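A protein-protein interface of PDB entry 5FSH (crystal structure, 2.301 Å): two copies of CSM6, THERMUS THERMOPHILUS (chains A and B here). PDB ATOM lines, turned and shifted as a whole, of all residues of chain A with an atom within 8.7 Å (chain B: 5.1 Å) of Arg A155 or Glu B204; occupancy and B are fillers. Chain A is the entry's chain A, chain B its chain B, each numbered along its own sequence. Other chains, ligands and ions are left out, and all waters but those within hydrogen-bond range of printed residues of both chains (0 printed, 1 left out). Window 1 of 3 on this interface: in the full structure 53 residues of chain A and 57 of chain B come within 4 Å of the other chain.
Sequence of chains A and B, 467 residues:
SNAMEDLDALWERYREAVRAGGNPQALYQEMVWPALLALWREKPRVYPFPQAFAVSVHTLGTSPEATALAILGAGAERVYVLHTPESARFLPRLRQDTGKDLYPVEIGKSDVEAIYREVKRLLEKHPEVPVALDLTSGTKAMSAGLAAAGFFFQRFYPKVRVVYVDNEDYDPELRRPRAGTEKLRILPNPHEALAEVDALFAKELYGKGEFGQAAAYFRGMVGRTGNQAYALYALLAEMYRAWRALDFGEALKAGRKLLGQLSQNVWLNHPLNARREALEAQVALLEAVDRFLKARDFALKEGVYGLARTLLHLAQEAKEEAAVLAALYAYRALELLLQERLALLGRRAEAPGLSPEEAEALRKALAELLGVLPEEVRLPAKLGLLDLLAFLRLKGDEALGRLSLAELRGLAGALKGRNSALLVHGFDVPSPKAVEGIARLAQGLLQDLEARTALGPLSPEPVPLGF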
ATOM      1  N   LEU A 123      -2.929 -16.693   0.305  1.00  0.00           N
ATOM      2  CA  LEU A 123      -2.754 -17.934  -0.438  1.00  0.00           C
ATOM      3  C   LEU A 123      -3.472 -19.090   0.247  1.00  0.00           C
ATOM      4  O   LEU A 123      -4.029 -19.963  -0.431  1.00  0.00           O
ATOM      5  CB  LEU A 123      -1.263 -18.239  -0.621  1.00  0.00           C
ATOM      6  CG  LEU A 123      -0.556 -17.290  -1.596  1.00  0.00           C
ATOM      7  CD1 LEU A 123       0.897 -17.685  -1.756  1.00  0.00           C
ATOM      8  CD2 LEU A 123      -1.269 -17.262  -2.944  1.00  0.00           C
ATOM      9  N   ALA A 148       9.796 -11.715  -2.917  1.00  0.00           N
ATOM     10  CA  ALA A 148      10.368 -12.802  -2.131  1.00  0.00           C
ATOM     11  C   ALA A 148       9.279 -13.727  -1.594  1.00  0.00           C
ATOM     12  O   ALA A 148       9.436 -14.953  -1.600  1.00  0.00           O
ATOM     13  CB  ALA A 148      11.202 -12.227  -0.986  1.00  0.00           C
ATOM     14  N   ALA A 149       8.165 -13.160  -1.135  1.00  0.00           N
ATOM     15  CA  ALA A 149       7.038 -13.981  -0.704  1.00  0.00           C
ATOM     16  C   ALA A 149       6.521 -14.834  -1.850  1.00  0.00           C
ATOM     17  O   ALA A 149       6.328 -16.040  -1.698  1.00  0.00           O
ATOM     18  CB  ALA A 149       5.919 -13.097  -0.140  1.00  0.00           C
ATOM     19  N   GLY A 150       6.295 -14.220  -3.011  1.00  0.00           N
ATOM     20  CA  GLY A 150       5.765 -14.971  -4.137  1.00  0.00           C
ATOM     21  C   GLY A 150       6.645 -16.140  -4.526  1.00  0.00           C
ATOM     22  O   GLY A 150       6.169 -17.269  -4.695  1.00  0.00           O
ATOM     23  N   PHE A 151       7.949 -15.887  -4.667  1.00  0.00           N
ATOM     24  CA  PHE A 151       8.839 -16.948  -5.121  1.00  0.00           C
ATOM     25  C   PHE A 151       9.007 -18.015  -4.052  1.00  0.00           C
ATOM     26  O   PHE A 151       9.097 -19.211  -4.359  1.00  0.00           O
ATOM     27  CB  PHE A 151      10.195 -16.365  -5.533  1.00  0.00           C
ATOM     28  CG  PHE A 151      10.133 -15.518  -6.776  1.00  0.00           C
ATOM     29  CD1 PHE A 151       9.310 -15.877  -7.837  1.00  0.00           C
ATOM     30  CD2 PHE A 151      10.877 -14.354  -6.880  1.00  0.00           C
ATOM     31  CE1 PHE A 151       9.247 -15.098  -8.988  1.00  0.00           C
ATOM     32  CE2 PHE A 151      10.820 -13.571  -8.026  1.00  0.00           C
ATOM     33  CZ  PHE A 151       9.999 -13.944  -9.080  1.00  0.00           C
ATOM     34  N   PHE A 152       9.035 -17.608  -2.787  1.00  0.00           N
ATOM     35  CA  PHE A 152       9.122 -18.608  -1.736  1.00  0.00           C
ATOM     36  C   PHE A 152       7.877 -19.487  -1.716  1.00  0.00           C
ATOM     37  O   PHE A 152       7.979 -20.717  -1.664  1.00  0.00           O
ATOM     38  CB  PHE A 152       9.331 -17.950  -0.377  1.00  0.00           C
ATOM     39  CG  PHE A 152       9.229 -18.921   0.751  1.00  0.00           C
ATOM     40  CD1 PHE A 152      10.228 -19.865   0.956  1.00  0.00           C
ATOM     41  CD2 PHE A 152       8.113 -18.941   1.569  1.00  0.00           C
ATOM     42  CE1 PHE A 152      10.128 -20.787   1.979  1.00  0.00           C
ATOM     43  CE2 PHE A 152       8.008 -19.858   2.601  1.00  0.00           C
ATOM     44  CZ  PHE A 152       9.017 -20.782   2.805  1.00  0.00           C
ATOM     45  N   PHE A 153       6.693 -18.878  -1.787  1.00  0.00           N
ATOM     46  CA  PHE A 153       5.445 -19.625  -1.672  1.00  0.00           C
ATOM     47  C   PHE A 153       5.071 -20.367  -2.944  1.00  0.00           C
ATOM     48  O   PHE A 153       4.145 -21.184  -2.904  1.00  0.00           O
ATOM     49  CB  PHE A 153       4.296 -18.700  -1.260  1.00  0.00           C
ATOM     50  CG  PHE A 153       4.293 -18.381   0.196  1.00  0.00           C
ATOM     51  CD1 PHE A 153       4.042 -19.372   1.133  1.00  0.00           C
ATOM     52  CD2 PHE A 153       4.554 -17.099   0.632  1.00  0.00           C
ATOM     53  CE1 PHE A 153       4.051 -19.085   2.482  1.00  0.00           C
ATOM     54  CE2 PHE A 153       4.568 -16.801   1.976  1.00  0.00           C
ATOM     55  CZ  PHE A 153       4.315 -17.797   2.908  1.00  0.00           C
ATOM     56  N   GLN A 154       5.762 -20.112  -4.061  1.00  0.00           N
ATOM     57  CA  GLN A 154       5.537 -20.917  -5.260  1.00  0.00           C
ATOM     58  C   GLN A 154       5.823 -22.391  -5.006  1.00  0.00           C
ATOM     59  O   GLN A 154       5.270 -23.257  -5.690  1.00  0.00           O
ATOM     60  CB  GLN A 154       6.402 -20.404  -6.410  1.00  0.00           C
ATOM     61  CG  GLN A 154       5.638 -19.886  -7.612  1.00  0.00           C
ATOM     62  CD  GLN A 154       6.527 -19.092  -8.551  1.00  0.00           C
ATOM     63  OE1 GLN A 154       7.749 -19.118  -8.424  1.00  0.00           O
ATOM     64  NE2 GLN A 154       5.921 -18.372  -9.486  1.00  0.00           N
ATOM     65  N   ARG A 155       6.688 -22.694  -4.039  1.00  0.00           N
ATOM     66  CA  ARG A 155       6.985 -24.084  -3.708  1.00  0.00           C
ATOM     67  C   ARG A 155       5.732 -24.836  -3.264  1.00  0.00           C
ATOM     68  O   ARG A 155       5.573 -26.025  -3.564  1.00  0.00           O
ATOM     69  CB  ARG A 155       8.071 -24.124  -2.629  1.00  0.00           C
ATOM     70  CG  ARG A 155       8.361 -25.478  -2.026  1.00  0.00           C
ATOM     71  CD  ARG A 155       9.624 -25.393  -1.182  1.00  0.00           C
ATOM     72  NE  ARG A 155       9.864 -26.598  -0.393  1.00  0.00           N
ATOM     73  CZ  ARG A 155      10.963 -26.804   0.324  1.00  0.00           C
ATOM     74  NH1 ARG A 155      11.916 -25.886   0.339  1.00  0.00           N
ATOM     75  NH2 ARG A 155      11.111 -27.918   1.023  1.00  0.00           N
ATOM     76  N   PHE A 156       4.819 -24.153  -2.568  1.00  0.00           N
ATOM     77  CA  PHE A 156       3.586 -24.769  -2.094  1.00  0.00           C
ATOM     78  C   PHE A 156       2.341 -24.300  -2.832  1.00  0.00           C
ATOM     79  O   PHE A 156       1.298 -24.950  -2.721  1.00  0.00           O
ATOM     80  CB  PHE A 156       3.399 -24.513  -0.590  1.00  0.00           C
ATOM     81  CG  PHE A 156       4.663 -24.636   0.203  1.00  0.00           C
ATOM     82  CD1 PHE A 156       5.107 -25.870   0.652  1.00  0.00           C
ATOM     83  CD2 PHE A 156       5.420 -23.513   0.485  1.00  0.00           C
ATOM     84  CE1 PHE A 156       6.287 -25.976   1.373  1.00  0.00           C
ATOM     85  CE2 PHE A 156       6.596 -23.607   1.201  1.00  0.00           C
ATOM     86  CZ  PHE A 156       7.034 -24.838   1.648  1.00  0.00           C
ATOM     87  N   TYR A 157       2.425 -23.204  -3.582  1.00  0.00           N
ATOM     88  CA  TYR A 157       1.318 -22.690  -4.388  1.00  0.00           C
ATOM     89  C   TYR A 157       1.867 -22.389  -5.776  1.00  0.00           C
ATOM     90  O   TYR A 157       2.199 -21.238  -6.088  1.00  0.00           O
ATOM     91  CB  TYR A 157       0.698 -21.441  -3.761  1.00  0.00           C
ATOM     92  CG  TYR A 157       0.238 -21.607  -2.330  1.00  0.00           C
ATOM     93  CD1 TYR A 157       1.098 -21.353  -1.270  1.00  0.00           C
ATOM     94  CD2 TYR A 157      -1.066 -21.992  -2.038  1.00  0.00           C
ATOM     95  CE1 TYR A 157       0.683 -21.492   0.038  1.00  0.00           C
ATOM     96  CE2 TYR A 157      -1.495 -22.135  -0.736  1.00  0.00           C
ATOM     97  CZ  TYR A 157      -0.616 -21.884   0.304  1.00  0.00           C
ATOM     98  OH  TYR A 157      -1.033 -22.024   1.608  1.00  0.00           O
ATOM     99  N   PRO A 158       1.969 -23.404  -6.642  1.00  0.00           N
ATOM    100  CA  PRO A 158       2.716 -23.234  -7.902  1.00  0.00           C
ATOM    101  C   PRO A 158       2.010 -22.374  -8.932  1.00  0.00           C
ATOM    102  O   PRO A 158       2.599 -22.096  -9.984  1.00  0.00           O
ATOM    103  CB  PRO A 158       2.874 -24.673  -8.414  1.00  0.00           C
ATOM    104  CG  PRO A 158       2.545 -25.555  -7.233  1.00  0.00           C
ATOM    105  CD  PRO A 158       1.526 -24.791  -6.451  1.00  0.00           C
ATOM    106  N   LYS A 159       0.775 -21.954  -8.679  1.00  0.00           N
ATOM    107  CA  LYS A 159       0.062 -21.063  -9.580  1.00  0.00           C
ATOM    108  C   LYS A 159       0.271 -19.590  -9.245  1.00  0.00           C
ATOM    109  O   LYS A 159      -0.208 -18.729  -9.985  1.00  0.00           O
ATOM    110  CB  LYS A 159      -1.431 -21.414  -9.584  1.00  0.00           C
ATOM    111  CG  LYS A 159      -1.738 -22.735 -10.290  1.00  0.00           C
ATOM    112  CD  LYS A 159      -3.061 -23.333  -9.837  1.00  0.00           C
ATOM    113  CE  LYS A 159      -3.340 -24.649 -10.552  1.00  0.00           C
ATOM    114  NZ  LYS A 159      -4.466 -25.398  -9.925  1.00  0.00           N
ATOM    115  N   VAL A 160       0.987 -19.284  -8.164  1.00  0.00           N
ATOM    116  CA  VAL A 160       1.427 -17.918  -7.904  1.00  0.00           C
ATOM    117  C   VAL A 160       2.401 -17.461  -8.984  1.00  0.00           C
ATOM    118  O   VAL A 160       3.313 -18.199  -9.377  1.00  0.00           O
ATOM    119  CB  VAL A 160       2.085 -17.831  -6.517  1.00  0.00           C
ATOM    120  CG1 VAL A 160       2.804 -16.510  -6.348  1.00  0.00           C
ATOM    121  CG2 VAL A 160       1.050 -18.000  -5.457  1.00  0.00           C
ATOM    122  N   ASN A 189      11.013 -16.635 -11.909  1.00  0.00           N
ATOM    123  CA  ASN A 189      11.598 -17.270 -10.734  1.00  0.00           C
ATOM    124  C   ASN A 189      13.069 -17.586 -11.004  1.00  0.00           C
ATOM    125  O   ASN A 189      13.417 -18.025 -12.105  1.00  0.00           O
ATOM    126  CB  ASN A 189      10.827 -18.553 -10.395  1.00  0.00           C
ATOM    127  CG  ASN A 189      11.107 -19.071  -8.988  1.00  0.00           C
ATOM    128  OD1 ASN A 189      12.223 -18.967  -8.477  1.00  0.00           O
ATOM    129  ND2 ASN A 189      10.085 -19.651  -8.362  1.00  0.00           N
ATOM    130  N   PHE A 201      20.786 -28.158  -6.748  1.00  0.00           N
ATOM    131  CA  PHE A 201      19.788 -29.069  -6.202  1.00  0.00           C
ATOM    132  C   PHE A 201      20.290 -30.501  -6.261  1.00  0.00           C
ATOM    133  O   PHE A 201      20.261 -31.231  -5.257  1.00  0.00           O
ATOM    134  CB  PHE A 201      18.475 -28.933  -6.972  1.00  0.00           C
ATOM    135  CG  PHE A 201      17.702 -27.693  -6.642  1.00  0.00           C
ATOM    136  CD1 PHE A 201      17.986 -26.489  -7.270  1.00  0.00           C
ATOM    137  CD2 PHE A 201      16.680 -27.735  -5.716  1.00  0.00           C
ATOM    138  CE1 PHE A 201      17.266 -25.350  -6.972  1.00  0.00           C
ATOM    139  CE2 PHE A 201      15.954 -26.596  -5.415  1.00  0.00           C
ATOM    140  CZ  PHE A 201      16.248 -25.403  -6.044  1.00  0.00           C
ATOM    141  N   GLU A 204      22.873 -31.217  -3.724  1.00  0.00           N
ATOM    142  CA  GLU A 204      22.252 -31.326  -2.413  1.00  0.00           C
ATOM    143  C   GLU A 204      21.663 -32.718  -2.228  1.00  0.00           C
ATOM    144  O   GLU A 204      21.978 -33.419  -1.258  1.00  0.00           O
ATOM    145  CB  GLU A 204      21.187 -30.237  -2.264  1.00  0.00           C
ATOM    146  CG  GLU A 204      20.613 -30.073  -0.870  1.00  0.00           C
ATOM    147  CD  GLU A 204      19.673 -28.882  -0.794  1.00  0.00           C
ATOM    148  OE1 GLU A 204      18.466 -29.060  -1.047  1.00  0.00           O
ATOM    149  OE2 GLU A 204      20.146 -27.761  -0.500  1.00  0.00           O
ATOM    150  N   LYS A 208      22.635 -36.293   0.491  1.00  0.00           N
ATOM    151  CA  LYS A 208      21.725 -36.971   1.402  1.00  0.00           C
ATOM    152  C   LYS A 208      21.378 -38.383   0.951  1.00  0.00           C
ATOM    153  O   LYS A 208      20.481 -39.003   1.532  1.00  0.00           O
ATOM    154  CB  LYS A 208      20.444 -36.150   1.568  1.00  0.00           C
ATOM    155  CG  LYS A 208      20.689 -34.738   2.048  1.00  0.00           C
ATOM    156  CD  LYS A 208      19.443 -33.882   1.894  1.00  0.00           C
ATOM    157  CE  LYS A 208      19.580 -32.563   2.645  1.00  0.00           C
ATOM    158  NZ  LYS A 208      18.433 -31.647   2.380  1.00  0.00           N
ATOM    159  N   ARG B 155      19.733 -20.866   0.274  1.00  0.00           N
ATOM    160  CA  ARG B 155      19.688 -22.300   0.543  1.00  0.00           C
ATOM    161  C   ARG B 155      21.030 -22.978   0.274  1.00  0.00           C
ATOM    162  O   ARG B 155      21.358 -23.966   0.941  1.00  0.00           O
ATOM    163  CB  ARG B 155      18.563 -22.945  -0.287  1.00  0.00           C
ATOM    164  CG  ARG B 155      18.944 -24.214  -1.017  1.00  0.00           C
ATOM    165  CD  ARG B 155      18.008 -25.385  -0.722  1.00  0.00           C
ATOM    166  NE  ARG B 155      16.774 -25.335  -1.498  1.00  0.00           N
ATOM    167  CZ  ARG B 155      16.012 -26.394  -1.761  1.00  0.00           C
ATOM    168  NH1 ARG B 155      16.366 -27.595  -1.328  1.00  0.00           N
ATOM    169  NH2 ARG B 155      14.895 -26.255  -2.460  1.00  0.00           N
ATOM    170  N   LEU B 200       3.990 -25.696   6.879  1.00  0.00           N
ATOM    171  CA  LEU B 200       3.885 -26.023   5.460  1.00  0.00           C
ATOM    172  C   LEU B 200       4.924 -27.059   5.061  1.00  0.00           C
ATOM    173  O   LEU B 200       4.609 -28.019   4.343  1.00  0.00           O
ATOM    174  CB  LEU B 200       4.029 -24.761   4.607  1.00  0.00           C
ATOM    175  CG  LEU B 200       2.941 -23.693   4.738  1.00  0.00           C
ATOM    176  CD1 LEU B 200       2.964 -22.757   3.543  1.00  0.00           C
ATOM    177  CD2 LEU B 200       1.566 -24.324   4.903  1.00  0.00           C
ATOM    178  N   PHE B 201       6.161 -26.903   5.551  1.00  0.00           N
ATOM    179  CA  PHE B 201       7.194 -27.892   5.261  1.00  0.00           C
ATOM    180  C   PHE B 201       6.722 -29.275   5.679  1.00  0.00           C
ATOM    181  O   PHE B 201       6.764 -30.231   4.887  1.00  0.00           O
ATOM    182  CB  PHE B 201       8.494 -27.521   5.979  1.00  0.00           C
ATOM    183  CG  PHE B 201       9.171 -26.291   5.425  1.00  0.00           C
ATOM    184  CD1 PHE B 201       9.457 -26.187   4.074  1.00  0.00           C
ATOM    185  CD2 PHE B 201       9.528 -25.240   6.264  1.00  0.00           C
ATOM    186  CE1 PHE B 201      10.092 -25.049   3.565  1.00  0.00           C
ATOM    187  CE2 PHE B 201      10.156 -24.109   5.770  1.00  0.00           C
ATOM    188  CZ  PHE B 201      10.439 -24.009   4.418  1.00  0.00           C
ATOM    189  N   ALA B 202       6.203 -29.373   6.908  1.00  0.00           N
ATOM    190  CA  ALA B 202       5.649 -30.622   7.412  1.00  0.00           C
ATOM    191  C   ALA B 202       4.662 -31.217   6.424  1.00  0.00           C
ATOM    192  O   ALA B 202       4.781 -32.388   6.036  1.00  0.00           O
ATOM    193  CB  ALA B 202       4.975 -30.380   8.763  1.00  0.00           C
ATOM    194  N   LYS B 203       3.703 -30.404   5.968  1.00  0.00           N
ATOM    195  CA  LYS B 203       2.671 -30.936   5.088  1.00  0.00           C
ATOM    196  C   LYS B 203       3.310 -31.542   3.850  1.00  0.00           C
ATOM    197  O   LYS B 203       3.001 -32.679   3.465  1.00  0.00           O
ATOM    198  CB  LYS B 203       1.667 -29.843   4.722  1.00  0.00           C
ATOM    199  CG  LYS B 203       0.541 -30.325   3.826  1.00  0.00           C
ATOM    200  CD  LYS B 203      -0.441 -29.215   3.496  1.00  0.00           C
ATOM    201  CE  LYS B 203      -1.436 -29.682   2.443  1.00  0.00           C
ATOM    202  NZ  LYS B 203      -2.373 -28.609   2.010  1.00  0.00           N
ATOM    203  N   GLU B 204       4.289 -30.837   3.281  1.00  0.00           N
ATOM    204  CA  GLU B 204       4.949 -31.336   2.082  1.00  0.00           C
ATOM    205  C   GLU B 204       5.601 -32.686   2.357  1.00  0.00           C
ATOM    206  O   GLU B 204       5.402 -33.652   1.608  1.00  0.00           O
ATOM    207  CB  GLU B 204       5.981 -30.318   1.585  1.00  0.00           C
ATOM    208  CG  GLU B 204       6.779 -30.769   0.377  1.00  0.00           C
ATOM    209  CD  GLU B 204       7.966 -29.864   0.092  1.00  0.00           C
ATOM    210  OE1 GLU B 204       7.765 -28.761  -0.456  1.00  0.00           O
ATOM    211  OE2 GLU B 204       9.101 -30.257   0.433  1.00  0.00           O
ATOM    212  N   LEU B 205       6.336 -32.787   3.469  1.00  0.00           N
ATOM    213  CA  LEU B 205       6.961 -34.059   3.811  1.00  0.00           C
ATOM    214  C   LEU B 205       5.900 -35.131   3.993  1.00  0.00           C
ATOM    215  O   LEU B 205       6.027 -36.248   3.475  1.00  0.00           O
ATOM    216  CB  LEU B 205       7.808 -33.908   5.073  1.00  0.00           C
ATOM    217  CG  LEU B 205       9.110 -33.129   4.895  1.00  0.00           C
ATOM    218  CD1 LEU B 205       9.637 -32.696   6.247  1.00  0.00           C
ATOM    219  CD2 LEU B 205      10.153 -33.965   4.165  1.00  0.00           C
ATOM    220  N   TYR B 206       4.812 -34.781   4.684  1.00  0.00           N
ATOM    221  CA  TYR B 206       3.728 -35.732   4.881  1.00  0.00           C
ATOM    222  C   TYR B 206       3.185 -36.199   3.542  1.00  0.00           C
ATOM    223  O   TYR B 206       2.852 -37.377   3.371  1.00  0.00           O
ATOM    224  CB  TYR B 206       2.635 -35.087   5.736  1.00  0.00           C
ATOM    225  CG  TYR B 206       1.459 -35.967   6.068  1.00  0.00           C
ATOM    226  CD1 TYR B 206       0.349 -36.021   5.235  1.00  0.00           C
ATOM    227  CD2 TYR B 206       1.440 -36.719   7.234  1.00  0.00           C
ATOM    228  CE1 TYR B 206      -0.734 -36.815   5.542  1.00  0.00           C
ATOM    229  CE2 TYR B 206       0.357 -37.516   7.552  1.00  0.00           C
ATOM    230  CZ  TYR B 206      -0.724 -37.561   6.703  1.00  0.00           C
ATOM    231  OH  TYR B 206      -1.805 -38.348   7.017  1.00  0.00           O
ATOM    232  N   GLY B 207       3.120 -35.293   2.566  1.00  0.00           N
ATOM    233  CA  GLY B 207       2.616 -35.669   1.260  1.00  0.00           C
ATOM    234  C   GLY B 207       3.532 -36.605   0.509  1.00  0.00           C
ATOM    235  O   GLY B 207       3.052 -37.413  -0.291  1.00  0.00           O
ATOM    236  N   LYS B 208       4.838 -36.533   0.769  1.00  0.00           N
ATOM    237  CA  LYS B 208       5.803 -37.355   0.056  1.00  0.00           C
ATOM    238  C   LYS B 208       6.063 -38.698   0.725  1.00  0.00           C
ATOM    239  O   LYS B 208       6.844 -39.497   0.195  1.00  0.00           O
ATOM    240  CB  LYS B 208       7.126 -36.597  -0.095  1.00  0.00           C
ATOM    241  CG  LYS B 208       7.047 -35.406  -1.031  1.00  0.00           C
ATOM    242  CD  LYS B 208       8.331 -34.593  -1.001  1.00  0.00           C
ATOM    243  CE  LYS B 208       8.366 -33.594  -2.149  1.00  0.00           C
ATOM    244  NZ  LYS B 208       9.517 -32.650  -2.056  1.00  0.00           N
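Among the printed residues, merely in contact across the chains: Phe A201 with Arg B155 (3.2 Å), Phe A156 with Phe B201 (3.6 Å), Phe A156 with Glu B204 (3.6 Å), Arg A155 with Phe B201 (3.8 Å), Phe A152 with Phe B201 (3.9 Å), Phe A153 with Leu B200 (3.97 Å) and Phe A156 with Leu B200 (3.98 Å).
Of the 10 printed residues of chain B, 4 touch a printed residue of chain A. Printed residues of chain A that touch a printed residue of chain B: Phe A152, Phe A153, Arg A155, Phe A156, Phe A201 and Glu A204. Among the printed residues, 9 pairs touch across the chains.
OE2 of Glu B204 lies within salt-bridge range of NZ of Lys B208.
OE1 of Glu A204 lies within salt-bridge range of NH1 of Arg B155, at 2.6 Å. NE of Arg A155 lies within salt-bridge range of OE1 of Glu B204.
Arg A155 touches Phe B201, and with the chains exchanged Phe A201 touches Arg B155. Arg A155 touches Glu B204, and with the chains exchanged Glu A204 touches Arg B155. 4 positions are printed for both chains. Of the 9 pairs that touch across the chains among the printed residues, 4 have their exchanged pair printed and touching as well.
Arg A155 touches two residues of chain B. Of the printed residues of chain B, Phe A156 touches Leu B200 (3.98 Å), Phe B201 (3.6 Å) and Glu B204 (3.6 Å). Of the printed residues of chain B, Glu A204 touches Arg B155 (2.6 Å). Of the printed residues of chain B, Phe A201 touches Arg B155. Of the printed residues of chain A, Phe B201 touches Phe A152 (3.9 Å), Arg A155 (3.8 Å) and Phe A156 (3.6 Å). Printed residues of chain B within 4 Å of Phe A152: Phe B201. Asn A189 touches none of the printed residues of chain B. The nearest residue of chain B that does not touch Arg A155 is Arg B155 (4.1 Å).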
